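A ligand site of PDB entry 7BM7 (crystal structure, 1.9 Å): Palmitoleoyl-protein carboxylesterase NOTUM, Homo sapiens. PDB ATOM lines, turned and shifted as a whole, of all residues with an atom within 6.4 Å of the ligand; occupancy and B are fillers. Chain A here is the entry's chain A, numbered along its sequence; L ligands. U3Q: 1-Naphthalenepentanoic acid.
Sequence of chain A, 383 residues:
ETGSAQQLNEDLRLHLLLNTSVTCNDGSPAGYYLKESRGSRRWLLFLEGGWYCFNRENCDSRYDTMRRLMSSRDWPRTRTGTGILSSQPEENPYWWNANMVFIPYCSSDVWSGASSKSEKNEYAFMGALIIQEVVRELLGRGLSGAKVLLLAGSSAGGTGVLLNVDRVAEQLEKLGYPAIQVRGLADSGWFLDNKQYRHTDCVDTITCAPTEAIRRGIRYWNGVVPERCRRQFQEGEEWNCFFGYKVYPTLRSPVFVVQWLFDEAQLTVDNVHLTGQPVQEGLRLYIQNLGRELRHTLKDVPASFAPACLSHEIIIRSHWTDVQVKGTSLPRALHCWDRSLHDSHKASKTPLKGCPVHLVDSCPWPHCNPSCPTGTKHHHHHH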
ATOM      1  N   GLY A  49       5.893  21.910  18.955  1.00  0.00           N
ATOM      2  CA  GLY A  49       6.198  22.219  20.339  1.00  0.00           C
ATOM      3  C   GLY A  49       7.695  22.396  20.574  1.00  0.00           C
ATOM      4  O   GLY A  49       8.487  22.490  19.646  1.00  0.00           O
ATOM      5  N   GLY A  50       8.057  22.455  21.861  1.00  0.00           N
ATOM      6  CA  GLY A  50       9.451  22.539  22.238  1.00  0.00           C
ATOM      7  C   GLY A  50       9.776  23.509  23.358  1.00  0.00           C
ATOM      8  O   GLY A  50      10.704  24.306  23.233  1.00  0.00           O
ATOM      9  N   TRP A  51       9.002  23.441  24.445  1.00  0.00           N
ATOM     10  CA  TRP A  51       9.231  24.217  25.683  1.00  0.00           C
ATOM     11  C   TRP A  51       9.119  25.713  25.370  1.00  0.00           C
ATOM     12  O   TRP A  51       8.228  26.128  24.602  1.00  0.00           O
ATOM     13  CB  TRP A  51      10.548  23.769  26.313  1.00  0.00           C
ATOM     14  CG  TRP A  51      10.458  22.390  26.911  1.00  0.00           C
ATOM     15  CD1 TRP A  51      10.827  21.213  26.323  1.00  0.00           C
ATOM     16  CD2 TRP A  51       9.943  22.037  28.209  1.00  0.00           C
ATOM     17  NE1 TRP A  51      10.584  20.152  27.184  1.00  0.00           N
ATOM     18  CE2 TRP A  51      10.039  20.635  28.339  1.00  0.00           C
ATOM     19  CE3 TRP A  51       9.426  22.774  29.270  1.00  0.00           C
ATOM     20  CZ2 TRP A  51       9.635  19.949  29.492  1.00  0.00           C
ATOM     21  CZ3 TRP A  51       9.028  22.100  30.408  1.00  0.00           C
ATOM     22  CH2 TRP A  51       9.137  20.708  30.511  1.00  0.00           C
ATOM     23  N   TYR A  52       9.974  26.557  25.958  1.00  0.00           N
ATOM     24  CA  TYR A  52       9.907  27.997  25.841  1.00  0.00           C
ATOM     25  C   TYR A  52      11.077  28.600  26.602  1.00  0.00           C
ATOM     26  O   TYR A  52      11.849  27.867  27.223  1.00  0.00           O
ATOM     27  CB  TYR A  52       8.581  28.554  26.394  1.00  0.00           C
ATOM     28  CG  TYR A  52       8.274  28.107  27.811  1.00  0.00           C
ATOM     29  CD1 TYR A  52       8.787  28.796  28.895  1.00  0.00           C
ATOM     30  CD2 TYR A  52       7.451  27.008  28.052  1.00  0.00           C
ATOM     31  CE1 TYR A  52       8.509  28.407  30.195  1.00  0.00           C
ATOM     32  CE2 TYR A  52       7.166  26.603  29.351  1.00  0.00           C
ATOM     33  CZ  TYR A  52       7.695  27.312  30.417  1.00  0.00           C
ATOM     34  OH  TYR A  52       7.419  26.928  31.710  1.00  0.00           O
ATOM     35  N   TYR A 105       7.932  26.042  15.270  1.00  0.00           N
ATOM     36  CA  TYR A 105       7.881  26.821  16.517  1.00  0.00           C
ATOM     37  C   TYR A 105       9.194  27.580  16.630  1.00  0.00           C
ATOM     38  O   TYR A 105      10.234  26.993  16.945  1.00  0.00           O
ATOM     39  CB  TYR A 105       7.650  25.861  17.674  1.00  0.00           C
ATOM     40  CG  TYR A 105       7.573  26.440  19.084  1.00  0.00           C
ATOM     41  CD1 TYR A 105       6.893  27.622  19.366  1.00  0.00           C
ATOM     42  CD2 TYR A 105       8.143  25.745  20.153  1.00  0.00           C
ATOM     43  CE1 TYR A 105       6.807  28.109  20.674  1.00  0.00           C
ATOM     44  CE2 TYR A 105       8.053  26.223  21.451  1.00  0.00           C
ATOM     45  CZ  TYR A 105       7.396  27.403  21.715  1.00  0.00           C
ATOM     46  OH  TYR A 105       7.337  27.858  22.993  1.00  0.00           O
ATOM     47  N   VAL A 110       5.202  29.664  23.729  1.00  0.00           N
ATOM     48  CA  VAL A 110       3.997  28.832  23.794  1.00  0.00           C
ATOM     49  C   VAL A 110       2.931  29.401  22.860  1.00  0.00           C
ATOM     50  O   VAL A 110       1.714  29.253  23.091  1.00  0.00           O
ATOM     51  CB  VAL A 110       3.478  28.700  25.252  1.00  0.00           C
ATOM     52  CG1 VAL A 110       2.523  27.526  25.388  1.00  0.00           C
ATOM     53  CG2 VAL A 110       4.657  28.518  26.229  1.00  0.00           C
ATOM     54  N   SER A 154       1.279  19.858  19.201  1.00  0.00           N
ATOM     55  CA  SER A 154       1.794  18.942  20.207  1.00  0.00           C
ATOM     56  C   SER A 154       2.622  19.707  21.226  1.00  0.00           C
ATOM     57  O   SER A 154       3.381  20.627  20.859  1.00  0.00           O
ATOM     58  CB  SER A 154       2.635  17.821  19.580  1.00  0.00           C
ATOM     59  OG  SER A 154       1.878  17.015  18.687  1.00  0.00           O
ATOM     60  N   SER A 155       2.474  19.339  22.496  1.00  0.00           N
ATOM     61  CA  SER A 155       3.335  19.867  23.577  1.00  0.00           C
ATOM     62  C   SER A 155       3.083  21.365  23.706  1.00  0.00           C
ATOM     63  O   SER A 155       1.915  21.775  23.840  1.00  0.00           O
ATOM     64  CB  SER A 155       4.777  19.479  23.293  1.00  0.00           C
ATOM     65  OG  SER A 155       4.886  18.103  23.368  1.00  0.00           O
ATOM     66  N   ALA A 156       4.100  22.225  23.662  1.00  0.00           N
ATOM     67  CA  ALA A 156       3.831  23.664  23.645  1.00  0.00           C
ATOM     68  C   ALA A 156       2.905  24.044  22.506  1.00  0.00           C
ATOM     69  O   ALA A 156       2.189  25.036  22.599  1.00  0.00           O
ATOM     70  CB  ALA A 156       5.125  24.485  23.537  1.00  0.00           C
ATOM     71  N   GLY A 157       2.904  23.263  21.412  1.00  0.00           N
ATOM     72  CA  GLY A 157       1.983  23.549  20.331  1.00  0.00           C
ATOM     73  C   GLY A 157       0.559  23.154  20.651  1.00  0.00           C
ATOM     74  O   GLY A 157      -0.393  23.749  20.122  1.00  0.00           O
ATOM     75  N   THR A 159      -0.741  23.422  23.750  1.00  0.00           N
ATOM     76  CA  THR A 159      -1.219  24.588  24.489  1.00  0.00           C
ATOM     77  C   THR A 159      -1.466  25.767  23.547  1.00  0.00           C
ATOM     78  O   THR A 159      -2.426  26.538  23.736  1.00  0.00           O
ATOM     79  CB  THR A 159      -0.190  24.945  25.573  1.00  0.00           C
ATOM     80  OG1 THR A 159       0.148  23.764  26.321  1.00  0.00           O
ATOM     81  CG2 THR A 159      -0.720  26.042  26.517  1.00  0.00           C
ATOM     82  N   SER A 188      -0.997  16.729  24.110  1.00  0.00           N
ATOM     83  CA  SER A 188       0.026  16.852  25.139  1.00  0.00           C
ATOM     84  C   SER A 188       0.273  18.298  25.564  1.00  0.00           C
ATOM     85  O   SER A 188       1.394  18.676  25.930  1.00  0.00           O
ATOM     86  CB  SER A 188       1.344  16.210  24.703  1.00  0.00           C
ATOM     87  OG  SER A 188       1.152  14.854  24.343  1.00  0.00           O
ATOM     88  N   GLY A 189      -0.766  19.132  25.510  1.00  0.00           N
ATOM     89  CA  GLY A 189      -0.628  20.498  25.977  1.00  0.00           C
ATOM     90  C   GLY A 189      -1.573  20.834  27.111  1.00  0.00           C
ATOM     91  O   GLY A 189      -1.895  22.008  27.317  1.00  0.00           O
ATOM     92  N   PHE A 191      -1.975  20.715  30.911  1.00  0.00           N
ATOM     93  CA  PHE A 191      -1.120  20.602  32.078  1.00  0.00           C
ATOM     94  C   PHE A 191      -1.850  21.033  33.351  1.00  0.00           C
ATOM     95  O   PHE A 191      -2.858  21.734  33.309  1.00  0.00           O
ATOM     96  CB  PHE A 191       0.154  21.443  31.912  1.00  0.00           C
ATOM     97  CG  PHE A 191       1.003  20.983  30.778  1.00  0.00           C
ATOM     98  CD1 PHE A 191       1.030  21.690  29.586  1.00  0.00           C
ATOM     99  CD2 PHE A 191       1.725  19.795  30.876  1.00  0.00           C
ATOM    100  CE1 PHE A 191       1.810  21.255  28.514  1.00  0.00           C
ATOM    101  CE2 PHE A 191       2.495  19.353  29.807  1.00  0.00           C
ATOM    102  CZ  PHE A 191       2.531  20.085  28.626  1.00  0.00           C
ATOM    103  N   LEU A 192      -1.301  20.583  34.473  1.00  0.00           N
ATOM    104  CA  LEU A 192      -1.851  20.876  35.794  1.00  0.00           C
ATOM    105  C   LEU A 192      -0.909  21.807  36.534  1.00  0.00           C
ATOM    106  O   LEU A 192       0.312  21.586  36.541  1.00  0.00           O
ATOM    107  CB  LEU A 192      -2.057  19.595  36.600  1.00  0.00           C
ATOM    108  CG  LEU A 192      -2.977  18.523  35.995  1.00  0.00           C
ATOM    109  CD1 LEU A 192      -3.130  17.354  36.961  1.00  0.00           C
ATOM    110  CD2 LEU A 192      -4.353  19.106  35.663  1.00  0.00           C
ATOM    111  N   PRO A 210       5.589  25.246  36.849  1.00  0.00           N
ATOM    112  CA  PRO A 210       5.088  25.923  35.632  1.00  0.00           C
ATOM    113  C   PRO A 210       4.492  27.298  35.898  1.00  0.00           C
ATOM    114  O   PRO A 210       4.687  28.205  35.071  1.00  0.00           O
ATOM    115  CB  PRO A 210       4.027  24.949  35.093  1.00  0.00           C
ATOM    116  CG  PRO A 210       4.113  23.717  35.950  1.00  0.00           C
ATOM    117  CD  PRO A 210       4.745  24.113  37.242  1.00  0.00           C
ATOM    118  N   ILE A 214       5.465  30.600  33.628  1.00  0.00           N
ATOM    119  CA  ILE A 214       4.504  31.206  32.721  1.00  0.00           C
ATOM    120  C   ILE A 214       4.193  32.662  33.113  1.00  0.00           C
ATOM    121  O   ILE A 214       4.064  33.532  32.246  1.00  0.00           O
ATOM    122  CB  ILE A 214       3.227  30.349  32.635  1.00  0.00           C
ATOM    123  CG1 ILE A 214       3.556  28.995  32.038  1.00  0.00           C
ATOM    124  CG2 ILE A 214       2.181  31.034  31.772  1.00  0.00           C
ATOM    125  CD1 ILE A 214       2.584  27.958  32.421  1.00  0.00           C
ATOM    126  N   PHE A 242      -3.126  29.532  30.355  1.00  0.00           N
ATOM    127  CA  PHE A 242      -2.202  28.568  29.774  1.00  0.00           C
ATOM    128  C   PHE A 242      -2.476  27.155  30.254  1.00  0.00           C
ATOM    129  O   PHE A 242      -1.828  26.217  29.783  1.00  0.00           O
ATOM    130  CB  PHE A 242      -0.750  28.932  30.115  1.00  0.00           C
ATOM    131  CG  PHE A 242      -0.211  30.054  29.288  1.00  0.00           C
ATOM    132  CD1 PHE A 242      -0.738  31.336  29.400  1.00  0.00           C
ATOM    133  CD2 PHE A 242       0.837  29.838  28.404  1.00  0.00           C
ATOM    134  CE1 PHE A 242      -0.228  32.371  28.626  1.00  0.00           C
ATOM    135  CE2 PHE A 242       1.336  30.864  27.633  1.00  0.00           C
ATOM    136  CZ  PHE A 242       0.803  32.131  27.744  1.00  0.00           C
ATOM    137  N   PHE A 243      -3.420  26.984  31.173  1.00  0.00           N
ATOM    138  CA  PHE A 243      -3.731  25.699  31.754  1.00  0.00           C
ATOM    139  C   PHE A 243      -5.057  25.204  31.183  1.00  0.00           C
ATOM    140  O   PHE A 243      -6.109  25.786  31.441  1.00  0.00           O
ATOM    141  CB  PHE A 243      -3.744  25.813  33.268  1.00  0.00           C
ATOM    142  CG  PHE A 243      -2.364  25.941  33.807  1.00  0.00           C
ATOM    143  CD1 PHE A 243      -1.772  27.179  33.871  1.00  0.00           C
ATOM    144  CD2 PHE A 243      -1.603  24.809  34.056  1.00  0.00           C
ATOM    145  CE1 PHE A 243      -0.465  27.318  34.286  1.00  0.00           C
ATOM    146  CE2 PHE A 243      -0.297  24.928  34.481  1.00  0.00           C
ATOM    147  CZ  PHE A 243       0.276  26.182  34.591  1.00  0.00           C
ATOM    148  N   ASP A 263       1.968  12.525  31.512  1.00  0.00           N
ATOM    149  CA  ASP A 263       2.801  13.200  30.529  1.00  0.00           C
ATOM    150  C   ASP A 263       4.216  13.452  31.071  1.00  0.00           C
ATOM    151  O   ASP A 263       4.390  13.939  32.181  1.00  0.00           O
ATOM    152  CB  ASP A 263       2.117  14.509  30.144  1.00  0.00           C
ATOM    153  CG  ASP A 263       2.846  15.217  29.057  1.00  0.00           C
ATOM    154  OD1 ASP A 263       2.608  14.886  27.877  1.00  0.00           O
ATOM    155  OD2 ASP A 263       3.689  16.061  29.401  1.00  0.00           O
ATOM    156  N   ALA A 265       6.465  15.652  30.236  1.00  0.00           N
ATOM    157  CA  ALA A 265       6.745  17.054  30.544  1.00  0.00           C
ATOM    158  C   ALA A 265       6.091  17.470  31.858  1.00  0.00           C
ATOM    159  O   ALA A 265       6.674  18.244  32.637  1.00  0.00           O
ATOM    160  CB  ALA A 265       6.263  17.942  29.394  1.00  0.00           C
ATOM    161  N   GLN A 266       4.880  16.992  32.122  1.00  0.00           N
ATOM    162  CA  GLN A 266       4.242  17.216  33.422  1.00  0.00           C
ATOM    163  C   GLN A 266       5.105  16.655  34.555  1.00  0.00           C
ATOM    164  O   GLN A 266       5.373  17.349  35.544  1.00  0.00           O
ATOM    165  CB  GLN A 266       2.849  16.595  33.415  1.00  0.00           C
ATOM    166  CG  GLN A 266       2.096  16.720  34.716  1.00  0.00           C
ATOM    167  CD  GLN A 266       1.464  18.092  34.902  1.00  0.00           C
ATOM    168  OE1 GLN A 266       0.637  18.525  34.077  1.00  0.00           O
ATOM    169  NE2 GLN A 266       1.824  18.778  35.982  1.00  0.00           N
ATOM    170  N   VAL A 269       8.355  18.848  35.115  1.00  0.00           N
ATOM    171  CA  VAL A 269       8.168  20.064  35.904  1.00  0.00           C
ATOM    172  C   VAL A 269       7.718  19.735  37.324  1.00  0.00           C
ATOM    173  O   VAL A 269       7.867  20.579  38.216  1.00  0.00           O
ATOM    174  CB  VAL A 269       7.199  21.061  35.223  1.00  0.00           C
ATOM    175  CG1 VAL A 269       7.718  21.415  33.835  1.00  0.00           C
ATOM    176  CG2 VAL A 269       5.775  20.528  35.143  1.00  0.00           C
ATOM    177  N   HIS A 312       5.103  11.296  25.791  1.00  0.00           N
ATOM    178  CA  HIS A 312       5.024  12.719  25.459  1.00  0.00           C
ATOM    179  C   HIS A 312       4.771  12.838  23.955  1.00  0.00           C
ATOM    180  O   HIS A 312       5.545  12.282  23.181  1.00  0.00           O
ATOM    181  CB  HIS A 312       6.313  13.465  25.845  1.00  0.00           C
ATOM    182  CG  HIS A 312       6.194  14.955  25.790  1.00  0.00           C
ATOM    183  ND1 HIS A 312       5.213  15.650  26.481  1.00  0.00           N
ATOM    184  CD2 HIS A 312       6.940  15.889  25.153  1.00  0.00           C
ATOM    185  CE1 HIS A 312       5.360  16.942  26.258  1.00  0.00           C
ATOM    186  NE2 HIS A 312       6.406  17.116  25.470  1.00  0.00           N
ATOM    187  N   GLU A 313       3.723  13.572  23.581  1.00  0.00           N
ATOM    188  CA  GLU A 313       3.284  13.770  22.192  1.00  0.00           C
ATOM    189  C   GLU A 313       2.742  12.499  21.550  1.00  0.00           C
ATOM    190  O   GLU A 313       3.077  11.389  21.983  1.00  0.00           O
ATOM    191  CB  GLU A 313       4.394  14.328  21.307  1.00  0.00           C
ATOM    192  CG  GLU A 313       5.121  15.488  21.913  1.00  0.00           C
ATOM    193  CD  GLU A 313       6.013  16.215  20.926  1.00  0.00           C
ATOM    194  OE1 GLU A 313       6.744  15.551  20.157  1.00  0.00           O
ATOM    195  OE2 GLU A 313       5.984  17.472  20.917  1.00  0.00           O
HETATM  196  C01 U3Q L   1       2.049  25.510  29.382  1.00  0.00           C
HETATM  197  C02 U3Q L   1       1.529  25.335  30.661  1.00  0.00           C
HETATM  198  C03 U3Q L   1       2.149  24.437  31.520  1.00  0.00           C
HETATM  199  C04 U3Q L   1       3.261  23.700  31.095  1.00  0.00           C
HETATM  200  C05 U3Q L   1       3.849  22.780  31.979  1.00  0.00           C
HETATM  201  C06 U3Q L   1       4.963  22.048  31.570  1.00  0.00           C
HETATM  202  C07 U3Q L   1       5.481  22.236  30.288  1.00  0.00           C
HETATM  203  C08 U3Q L   1       4.921  23.131  29.408  1.00  0.00           C
HETATM  204  C09 U3Q L   1       5.573  23.242  28.020  1.00  0.00           C
HETATM  205  C10 U3Q L   1       5.074  22.226  26.973  1.00  0.00           C
HETATM  206  C11 U3Q L   1       5.568  20.782  27.039  1.00  0.00           C
HETATM  207  C12 U3Q L   1       7.021  20.637  26.593  1.00  0.00           C
HETATM  208  C13 U3Q L   1       7.283  20.556  25.087  1.00  0.00           C
HETATM  209  C16 U3Q L   1       3.782  23.875  29.816  1.00  0.00           C
HETATM  210  C17 U3Q L   1       3.166  24.803  28.955  1.00  0.00           C
HETATM  211  O14 U3Q L   1       7.806  19.510  24.578  1.00  0.00           O
HETATM  212  O15 U3Q L   1       6.986  21.538  24.369  1.00  0.00           O
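C of Gly 49 touches O15 of the ligand, 3.95 Å away.
Tyr 52 touches the ligand (CE2 to C09, 3.95 Å).
Phe 191 touches the ligand (CD1 to C04, 3.4 Å).
Pro 210 touches the ligand.
CD1 of Ile 214 touches C02 of the ligand (3.3 Å).
O of Phe 242 touches C02 of the ligand, 3.6 Å away.
Phe 243 touches the ligand (CE2 to C03, 3.9 Å).
Ala 265 touches the ligand (CB to C11, 3.8 Å).
Val 269 touches the ligand (CG1 to C06, 3.6 Å).
Hydrophobic or aromatic side chains that line the ligand: Trp 51, Tyr 52, Ala 156, Phe 191, Pro 210, Ile 214, Phe 243, Ala 265, Val 269 and His 312.
The nearest printed residue that does not touch the ligand is Thr 159 (4.004 Å).
An oxygen (O15) of the ligand lies within hydrogen-bond range of the backbone NH of Ala 156 (3.0 Å).
NE2 of His 312 is in hydrogen-bond range of O14 of the ligand, at 2.9 Å.
The backbone NH (N) of Trp 51 sits at hydrogen-bond distance from an oxygen (O15) of the ligand (2.8 Å).
An oxygen (O14) of the ligand lies close to the side-chain hydroxyl (OG) of Ser 155 (3.5 Å).
N of Gly 50 lies within hydrogen-bond range of O15 of the ligand, 2.9 Å away.
O of Trp 51 lies within hydrogen-bond range of OH of Tyr 105 (2.5 Å).
N of Ala 265 sits at hydrogen-bond distance from OD2 of Asp 263, at 2.9 Å.
N of Gly 49 lies close to O of Ser 154 (3.4 Å).
ND1 of His 312 is in hydrogen-bond range of OD1 of Asp 263 (3.1 Å).
The side-chain hydroxyl (OG) of Ser 155 sits at hydrogen-bond distance from the side-chain carboxylate (OE2) of Glu 313 (2.8 Å).
A ring nitrogen (NE2) of His 312 lies within hydrogen-bond range of the side-chain hydroxyl (OG) of Ser 155, at 2.8 Å.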
